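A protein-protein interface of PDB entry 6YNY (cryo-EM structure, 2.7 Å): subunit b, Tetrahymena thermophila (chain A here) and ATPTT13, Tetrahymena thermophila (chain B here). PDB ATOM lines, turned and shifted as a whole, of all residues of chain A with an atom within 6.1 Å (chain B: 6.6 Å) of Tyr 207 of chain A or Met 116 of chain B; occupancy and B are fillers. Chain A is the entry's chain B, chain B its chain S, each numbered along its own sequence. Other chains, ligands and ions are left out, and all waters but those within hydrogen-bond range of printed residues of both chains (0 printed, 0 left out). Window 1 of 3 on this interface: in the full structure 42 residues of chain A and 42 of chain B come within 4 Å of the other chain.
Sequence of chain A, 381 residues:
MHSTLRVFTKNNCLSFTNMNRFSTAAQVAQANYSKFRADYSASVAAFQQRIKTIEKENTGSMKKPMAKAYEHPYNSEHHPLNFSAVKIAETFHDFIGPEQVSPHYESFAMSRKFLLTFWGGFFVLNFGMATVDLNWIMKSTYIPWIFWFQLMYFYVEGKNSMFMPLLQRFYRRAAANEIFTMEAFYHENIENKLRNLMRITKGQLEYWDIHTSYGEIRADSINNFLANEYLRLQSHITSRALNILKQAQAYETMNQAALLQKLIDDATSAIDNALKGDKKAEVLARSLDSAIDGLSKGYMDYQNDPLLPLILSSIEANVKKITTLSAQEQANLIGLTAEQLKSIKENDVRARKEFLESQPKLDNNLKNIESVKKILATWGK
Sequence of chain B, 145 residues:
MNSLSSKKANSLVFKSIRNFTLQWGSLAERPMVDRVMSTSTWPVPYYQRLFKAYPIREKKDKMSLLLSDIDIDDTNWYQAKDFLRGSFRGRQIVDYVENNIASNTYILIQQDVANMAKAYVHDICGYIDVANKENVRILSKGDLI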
ATOM      1  N   GLY A 203     -23.363 -33.615 -16.174  1.00  0.00           N
ATOM      2  CA  GLY A 203     -22.339 -32.610 -15.951  1.00  0.00           C
ATOM      3  C   GLY A 203     -22.910 -31.248 -15.603  1.00  0.00           C
ATOM      4  O   GLY A 203     -22.326 -30.505 -14.811  1.00  0.00           O
ATOM      5  N   GLN A 204     -24.052 -30.900 -16.193  1.00  0.00           N
ATOM      6  CA  GLN A 204     -24.683 -29.622 -15.893  1.00  0.00           C
ATOM      7  C   GLN A 204     -25.367 -29.623 -14.537  1.00  0.00           C
ATOM      8  O   GLN A 204     -25.518 -28.562 -13.924  1.00  0.00           O
ATOM      9  CB  GLN A 204     -25.691 -29.272 -16.983  1.00  0.00           C
ATOM     10  CG  GLN A 204     -25.062 -28.913 -18.305  1.00  0.00           C
ATOM     11  CD  GLN A 204     -24.366 -27.577 -18.271  1.00  0.00           C
ATOM     12  OE1 GLN A 204     -24.962 -26.561 -17.920  1.00  0.00           O
ATOM     13  NE2 GLN A 204     -23.093 -27.571 -18.630  1.00  0.00           N
ATOM     14  N   LEU A 205     -25.784 -30.788 -14.053  1.00  0.00           N
ATOM     15  CA  LEU A 205     -26.401 -30.880 -12.741  1.00  0.00           C
ATOM     16  C   LEU A 205     -25.391 -30.808 -11.606  1.00  0.00           C
ATOM     17  O   LEU A 205     -25.798 -30.766 -10.440  1.00  0.00           O
ATOM     18  CB  LEU A 205     -27.199 -32.177 -12.637  1.00  0.00           C
ATOM     19  CG  LEU A 205     -28.314 -32.335 -13.668  1.00  0.00           C
ATOM     20  CD1 LEU A 205     -28.893 -33.723 -13.617  1.00  0.00           C
ATOM     21  CD2 LEU A 205     -29.395 -31.320 -13.438  1.00  0.00           C
ATOM     22  N   GLU A 206     -24.094 -30.792 -11.912  1.00  0.00           N
ATOM     23  CA  GLU A 206     -23.080 -30.656 -10.876  1.00  0.00           C
ATOM     24  C   GLU A 206     -23.036 -29.253 -10.293  1.00  0.00           C
ATOM     25  O   GLU A 206     -22.548 -29.074  -9.174  1.00  0.00           O
ATOM     26  CB  GLU A 206     -21.707 -31.018 -11.436  1.00  0.00           C
ATOM     27  CG  GLU A 206     -21.599 -32.442 -11.930  1.00  0.00           C
ATOM     28  CD  GLU A 206     -20.236 -32.759 -12.506  1.00  0.00           C
ATOM     29  OE1 GLU A 206     -19.358 -31.871 -12.483  1.00  0.00           O
ATOM     30  OE2 GLU A 206     -20.041 -33.896 -12.982  1.00  0.00           O
ATOM     31  N   TYR A 207     -23.531 -28.256 -11.026  1.00  0.00           N
ATOM     32  CA  TYR A 207     -23.519 -26.889 -10.525  1.00  0.00           C
ATOM     33  C   TYR A 207     -24.554 -26.679  -9.430  1.00  0.00           C
ATOM     34  O   TYR A 207     -24.378 -25.807  -8.573  1.00  0.00           O
ATOM     35  CB  TYR A 207     -23.756 -25.916 -11.676  1.00  0.00           C
ATOM     36  CG  TYR A 207     -22.673 -25.935 -12.722  1.00  0.00           C
ATOM     37  CD1 TYR A 207     -22.630 -26.926 -13.686  1.00  0.00           C
ATOM     38  CD2 TYR A 207     -21.695 -24.956 -12.749  1.00  0.00           C
ATOM     39  CE1 TYR A 207     -21.641 -26.946 -14.641  1.00  0.00           C
ATOM     40  CE2 TYR A 207     -20.704 -24.967 -13.701  1.00  0.00           C
ATOM     41  CZ  TYR A 207     -20.682 -25.961 -14.646  1.00  0.00           C
ATOM     42  OH  TYR A 207     -19.691 -25.975 -15.597  1.00  0.00           O
ATOM     43  N   TRP A 208     -25.634 -27.458  -9.442  1.00  0.00           N
ATOM     44  CA  TRP A 208     -26.654 -27.331  -8.410  1.00  0.00           C
ATOM     45  C   TRP A 208     -26.248 -28.034  -7.126  1.00  0.00           C
ATOM     46  O   TRP A 208     -26.600 -27.573  -6.035  1.00  0.00           O
ATOM     47  CB  TRP A 208     -27.979 -27.885  -8.924  1.00  0.00           C
ATOM     48  CG  TRP A 208     -29.080 -27.863  -7.921  1.00  0.00           C
ATOM     49  CD1 TRP A 208     -29.667 -28.937  -7.332  1.00  0.00           C
ATOM     50  CD2 TRP A 208     -29.731 -26.707  -7.387  1.00  0.00           C
ATOM     51  NE1 TRP A 208     -30.645 -28.527  -6.466  1.00  0.00           N
ATOM     52  CE2 TRP A 208     -30.704 -27.160  -6.480  1.00  0.00           C
ATOM     53  CE3 TRP A 208     -29.586 -25.334  -7.586  1.00  0.00           C
ATOM     54  CZ2 TRP A 208     -31.525 -26.290  -5.775  1.00  0.00           C
ATOM     55  CZ3 TRP A 208     -30.400 -24.475  -6.888  1.00  0.00           C
ATOM     56  CH2 TRP A 208     -31.359 -24.954  -5.993  1.00  0.00           C
ATOM     57  N   ASP A 209     -25.511 -29.139  -7.229  1.00  0.00           N
ATOM     58  CA  ASP A 209     -25.045 -29.835  -6.039  1.00  0.00           C
ATOM     59  C   ASP A 209     -24.035 -29.004  -5.264  1.00  0.00           C
ATOM     60  O   ASP A 209     -23.874 -29.209  -4.056  1.00  0.00           O
ATOM     61  CB  ASP A 209     -24.429 -31.177  -6.426  1.00  0.00           C
ATOM     62  CG  ASP A 209     -25.399 -32.069  -7.172  1.00  0.00           C
ATOM     63  OD1 ASP A 209     -26.597 -31.725  -7.238  1.00  0.00           O
ATOM     64  OD2 ASP A 209     -24.963 -33.115  -7.698  1.00  0.00           O
ATOM     65  N   ILE A 210     -23.355 -28.078  -5.935  1.00  0.00           N
ATOM     66  CA  ILE A 210     -22.381 -27.220  -5.273  1.00  0.00           C
ATOM     67  C   ILE A 210     -23.079 -26.098  -4.517  1.00  0.00           C
ATOM     68  O   ILE A 210     -22.672 -25.731  -3.411  1.00  0.00           O
ATOM     69  CB  ILE A 210     -21.389 -26.671  -6.313  1.00  0.00           C
ATOM     70  CG1 ILE A 210     -20.574 -27.815  -6.913  1.00  0.00           C
ATOM     71  CG2 ILE A 210     -20.474 -25.643  -5.690  1.00  0.00           C
ATOM     72  CD1 ILE A 210     -19.742 -27.415  -8.100  1.00  0.00           C
ATOM     73  N   HIS A 211     -24.139 -25.540  -5.099  1.00  0.00           N
ATOM     74  CA  HIS A 211     -24.830 -24.422  -4.472  1.00  0.00           C
ATOM     75  C   HIS A 211     -25.610 -24.853  -3.239  1.00  0.00           C
ATOM     76  O   HIS A 211     -25.756 -24.069  -2.296  1.00  0.00           O
ATOM     77  CB  HIS A 211     -25.765 -23.767  -5.481  1.00  0.00           C
ATOM     78  CG  HIS A 211     -26.590 -22.659  -4.911  1.00  0.00           C
ATOM     79  ND1 HIS A 211     -26.033 -21.537  -4.337  1.00  0.00           N
ATOM     80  CD2 HIS A 211     -27.930 -22.498  -4.828  1.00  0.00           C
ATOM     81  CE1 HIS A 211     -26.996 -20.733  -3.925  1.00  0.00           C
ATOM     82  NE2 HIS A 211     -28.156 -21.292  -4.212  1.00  0.00           N
ATOM     83  N   THR A 212     -26.123 -26.083  -3.226  1.00  0.00           N
ATOM     84  CA  THR A 212     -26.905 -26.545  -2.088  1.00  0.00           C
ATOM     85  C   THR A 212     -26.070 -26.683  -0.824  1.00  0.00           C
ATOM     86  O   THR A 212     -26.637 -26.755   0.271  1.00  0.00           O
ATOM     87  CB  THR A 212     -27.561 -27.885  -2.407  1.00  0.00           C
ATOM     88  OG1 THR A 212     -26.573 -28.799  -2.895  1.00  0.00           O
ATOM     89  CG2 THR A 212     -28.648 -27.707  -3.445  1.00  0.00           C
ATOM     90  N   GLN B 110     -24.346 -23.901 -18.126  1.00  0.00           N
ATOM     91  CA  GLN B 110     -23.302 -23.491 -17.197  1.00  0.00           C
ATOM     92  C   GLN B 110     -21.983 -24.100 -17.654  1.00  0.00           C
ATOM     93  O   GLN B 110     -21.805 -25.321 -17.612  1.00  0.00           O
ATOM     94  CB  GLN B 110     -23.647 -23.917 -15.775  1.00  0.00           C
ATOM     95  CG  GLN B 110     -24.797 -23.144 -15.162  1.00  0.00           C
ATOM     96  CD  GLN B 110     -24.509 -21.667 -15.035  1.00  0.00           C
ATOM     97  OE1 GLN B 110     -25.314 -20.830 -15.443  1.00  0.00           O
ATOM     98  NE2 GLN B 110     -23.362 -21.336 -14.461  1.00  0.00           N
ATOM     99  N   GLN B 111     -21.063 -23.246 -18.092  1.00  0.00           N
ATOM    100  CA  GLN B 111     -19.729 -23.666 -18.483  1.00  0.00           C
ATOM    101  C   GLN B 111     -18.646 -22.998 -17.652  1.00  0.00           C
ATOM    102  O   GLN B 111     -17.464 -23.314 -17.831  1.00  0.00           O
ATOM    103  CB  GLN B 111     -19.493 -23.378 -19.972  1.00  0.00           C
ATOM    104  CG  GLN B 111     -19.508 -21.906 -20.357  1.00  0.00           C
ATOM    105  CD  GLN B 111     -20.899 -21.307 -20.347  1.00  0.00           C
ATOM    106  OE1 GLN B 111     -21.570 -21.285 -19.315  1.00  0.00           O
ATOM    107  NE2 GLN B 111     -21.345 -20.826 -21.501  1.00  0.00           N
ATOM    108  N   ASP B 112     -19.012 -22.089 -16.752  1.00  0.00           N
ATOM    109  CA  ASP B 112     -18.059 -21.458 -15.855  1.00  0.00           C
ATOM    110  C   ASP B 112     -18.785 -21.081 -14.573  1.00  0.00           C
ATOM    111  O   ASP B 112     -20.014 -20.991 -14.536  1.00  0.00           O
ATOM    112  CB  ASP B 112     -17.413 -20.228 -16.495  1.00  0.00           C
ATOM    113  CG  ASP B 112     -16.199 -19.747 -15.733  1.00  0.00           C
ATOM    114  OD1 ASP B 112     -15.892 -20.335 -14.676  1.00  0.00           O
ATOM    115  OD2 ASP B 112     -15.551 -18.784 -16.191  1.00  0.00           O
ATOM    116  N   VAL B 113     -18.005 -20.854 -13.520  1.00  0.00           N
ATOM    117  CA  VAL B 113     -18.556 -20.585 -12.198  1.00  0.00           C
ATOM    118  C   VAL B 113     -18.372 -19.114 -11.852  1.00  0.00           C
ATOM    119  O   VAL B 113     -18.302 -18.745 -10.675  1.00  0.00           O
ATOM    120  CB  VAL B 113     -17.906 -21.487 -11.134  1.00  0.00           C
ATOM    121  CG1 VAL B 113     -18.268 -22.932 -11.381  1.00  0.00           C
ATOM    122  CG2 VAL B 113     -16.403 -21.323 -11.144  1.00  0.00           C
ATOM    123  N   ALA B 114     -18.296 -18.265 -12.875  1.00  0.00           N
ATOM    124  CA  ALA B 114     -18.159 -16.833 -12.642  1.00  0.00           C
ATOM    125  C   ALA B 114     -19.374 -16.281 -11.911  1.00  0.00           C
ATOM    126  O   ALA B 114     -19.253 -15.663 -10.847  1.00  0.00           O
ATOM    127  CB  ALA B 114     -17.958 -16.107 -13.972  1.00  0.00           C
ATOM    128  N   ASN B 115     -20.564 -16.502 -12.470  1.00  0.00           N
ATOM    129  CA  ASN B 115     -21.786 -16.016 -11.845  1.00  0.00           C
ATOM    130  C   ASN B 115     -22.023 -16.629 -10.473  1.00  0.00           C
ATOM    131  O   ASN B 115     -22.759 -16.049  -9.668  1.00  0.00           O
ATOM    132  CB  ASN B 115     -22.979 -16.307 -12.751  1.00  0.00           C
ATOM    133  CG  ASN B 115     -23.067 -17.764 -13.146  1.00  0.00           C
ATOM    134  OD1 ASN B 115     -22.052 -18.449 -13.261  1.00  0.00           O
ATOM    135  ND2 ASN B 115     -24.283 -18.246 -13.360  1.00  0.00           N
ATOM    136  N   MET B 116     -21.423 -17.782 -10.185  1.00  0.00           N
ATOM    137  CA  MET B 116     -21.645 -18.450  -8.911  1.00  0.00           C
ATOM    138  C   MET B 116     -20.708 -17.925  -7.831  1.00  0.00           C
ATOM    139  O   MET B 116     -21.152 -17.583  -6.731  1.00  0.00           O
ATOM    140  CB  MET B 116     -21.465 -19.960  -9.077  1.00  0.00           C
ATOM    141  CG  MET B 116     -22.446 -20.592 -10.045  1.00  0.00           C
ATOM    142  SD  MET B 116     -22.048 -22.302 -10.438  1.00  0.00           S
ATOM    143  CE  MET B 116     -22.071 -23.031  -8.810  1.00  0.00           C
ATOM    144  N   ALA B 117     -19.411 -17.857  -8.130  1.00  0.00           N
ATOM    145  CA  ALA B 117     -18.453 -17.368  -7.146  1.00  0.00           C
ATOM    146  C   ALA B 117     -18.634 -15.879  -6.886  1.00  0.00           C
ATOM    147  O   ALA B 117     -18.443 -15.420  -5.755  1.00  0.00           O
ATOM    148  CB  ALA B 117     -17.030 -17.656  -7.616  1.00  0.00           C
ATOM    149  N   LYS B 118     -19.002 -15.117  -7.916  1.00  0.00           N
ATOM    150  CA  LYS B 118     -19.216 -13.685  -7.743  1.00  0.00           C
ATOM    151  C   LYS B 118     -20.310 -13.411  -6.722  1.00  0.00           C
ATOM    152  O   LYS B 118     -20.187 -12.500  -5.897  1.00  0.00           O
ATOM    153  CB  LYS B 118     -19.567 -13.053  -9.087  1.00  0.00           C
ATOM    154  CG  LYS B 118     -19.859 -11.567  -9.025  1.00  0.00           C
ATOM    155  CD  LYS B 118     -20.120 -11.008 -10.412  1.00  0.00           C
ATOM    156  CE  LYS B 118     -20.294  -9.502 -10.382  1.00  0.00           C
ATOM    157  NZ  LYS B 118     -20.600  -8.955 -11.732  1.00  0.00           N
ATOM    158  N   ALA B 119     -21.392 -14.188  -6.764  1.00  0.00           N
ATOM    159  CA  ALA B 119     -22.474 -14.005  -5.808  1.00  0.00           C
ATOM    160  C   ALA B 119     -22.109 -14.510  -4.421  1.00  0.00           C
ATOM    161  O   ALA B 119     -22.766 -14.130  -3.447  1.00  0.00           O
ATOM    162  CB  ALA B 119     -23.733 -14.711  -6.300  1.00  0.00           C
ATOM    163  N   TYR B 120     -21.085 -15.355  -4.309  1.00  0.00           N
ATOM    164  CA  TYR B 120     -20.670 -15.838  -2.999  1.00  0.00           C
ATOM    165  C   TYR B 120     -19.770 -14.832  -2.297  1.00  0.00           C
ATOM    166  O   TYR B 120     -19.910 -14.606  -1.090  1.00  0.00           O
ATOM    167  CB  TYR B 120     -19.952 -17.178  -3.139  1.00  0.00           C
ATOM    168  CG  TYR B 120     -20.784 -18.268  -3.769  1.00  0.00           C
ATOM    169  CD1 TYR B 120     -22.168 -18.239  -3.710  1.00  0.00           C
ATOM    170  CD2 TYR B 120     -20.181 -19.330  -4.425  1.00  0.00           C
ATOM    171  CE1 TYR B 120     -22.926 -19.236  -4.287  1.00  0.00           C
ATOM    172  CE2 TYR B 120     -20.930 -20.328  -5.003  1.00  0.00           C
ATOM    173  CZ  TYR B 120     -22.301 -20.278  -4.932  1.00  0.00           C
ATOM    174  OH  TYR B 120     -23.049 -21.275  -5.508  1.00  0.00           O
ATOM    175  N   VAL B 121     -18.842 -14.217  -3.032  1.00  0.00           N
ATOM    176  CA  VAL B 121     -17.986 -13.207  -2.423  1.00  0.00           C
ATOM    177  C   VAL B 121     -18.794 -11.966  -2.075  1.00  0.00           C
ATOM    178  O   VAL B 121     -18.503 -11.284  -1.086  1.00  0.00           O
ATOM    179  CB  VAL B 121     -16.807 -12.869  -3.354  1.00  0.00           C
ATOM    180  CG1 VAL B 121     -15.953 -14.102  -3.591  1.00  0.00           C
ATOM    181  CG2 VAL B 121     -17.304 -12.298  -4.668  1.00  0.00           C
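Among the printed residues, merely in contact across the chains: Tyr 207 of chain A with Gln 111 of chain B (3.7 Å), Tyr 207 of chain A with Val 113 of chain B (3.9 Å) and Tyr 207 of chain A with Met 116 of chain B (3.5 Å).
Hydrophobic or aromatic side chains of chain B within 4 Å of the printed part of chain A: Val 113, Met 116 and Tyr 120.
Along chain B the printed residues that touch a printed residue of chain A span positions 110 to 120.
Of the 10 printed residues of chain A, 3 touch a printed residue of chain B.
Among the printed residues, 6 pairs touch across the chains.
Among the printed residues, no Asp or Glu carboxylate lies within 4 Å of a Lys or Arg side-chain nitrogen of the other chain.
Gly 203 of chain A touches none of the printed residues of chain B.
Of the printed residues of chain B, Gln 204 of chain A touches Gln 110 (2.7 Å).
Tyr 207 of chain A touches just these residues of chain B: Gln 110, Gln 111, Val 113 and Met 116.
Asp 209 of chain A touches none of the printed residues of chain B.
Of the printed residues of chain B, His 211 of chain A touches Tyr 120.
Of the printed residues of chain A, Gln 110 of chain B touches Gln 204 (2.7 Å) and Tyr 207 (3.0 Å).
Of the printed residues of chain A, Val 113 of chain B touches Tyr 207.
Of the printed residues of chain A, Met 116 of chain B touches Tyr 207 (3.5 Å).
The nearest printed residue of chain A that does not touch Val 113 of chain B is Ile 210 of chain A (5.7 Å).
The side-chain hydroxyl of Tyr 120 of chain B sits at hydrogen-bond distance from a ring nitrogen (ND1) of His 211 of chain A, at 3.2 Å.
The backbone NH of Gln 110 of chain B sits at hydrogen-bond distance from the side-chain amide oxygen of Gln 204 of chain A (2.7 Å).
The side-chain hydroxyl of Tyr 207 of chain A lies within hydrogen-bond range of the backbone carbonyl oxygen of Gln 110 of chain B.
The backbone carbonyl oxygen of Asp 112 of chain B sits at hydrogen-bond distance from the side-chain amide nitrogen of Gln 110 of chain B.
The side-chain amide nitrogen (NE2) of Gln 110 of chain B lies within hydrogen-bond range of the side-chain amide oxygen (OD1) of Asn 115 of chain B.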
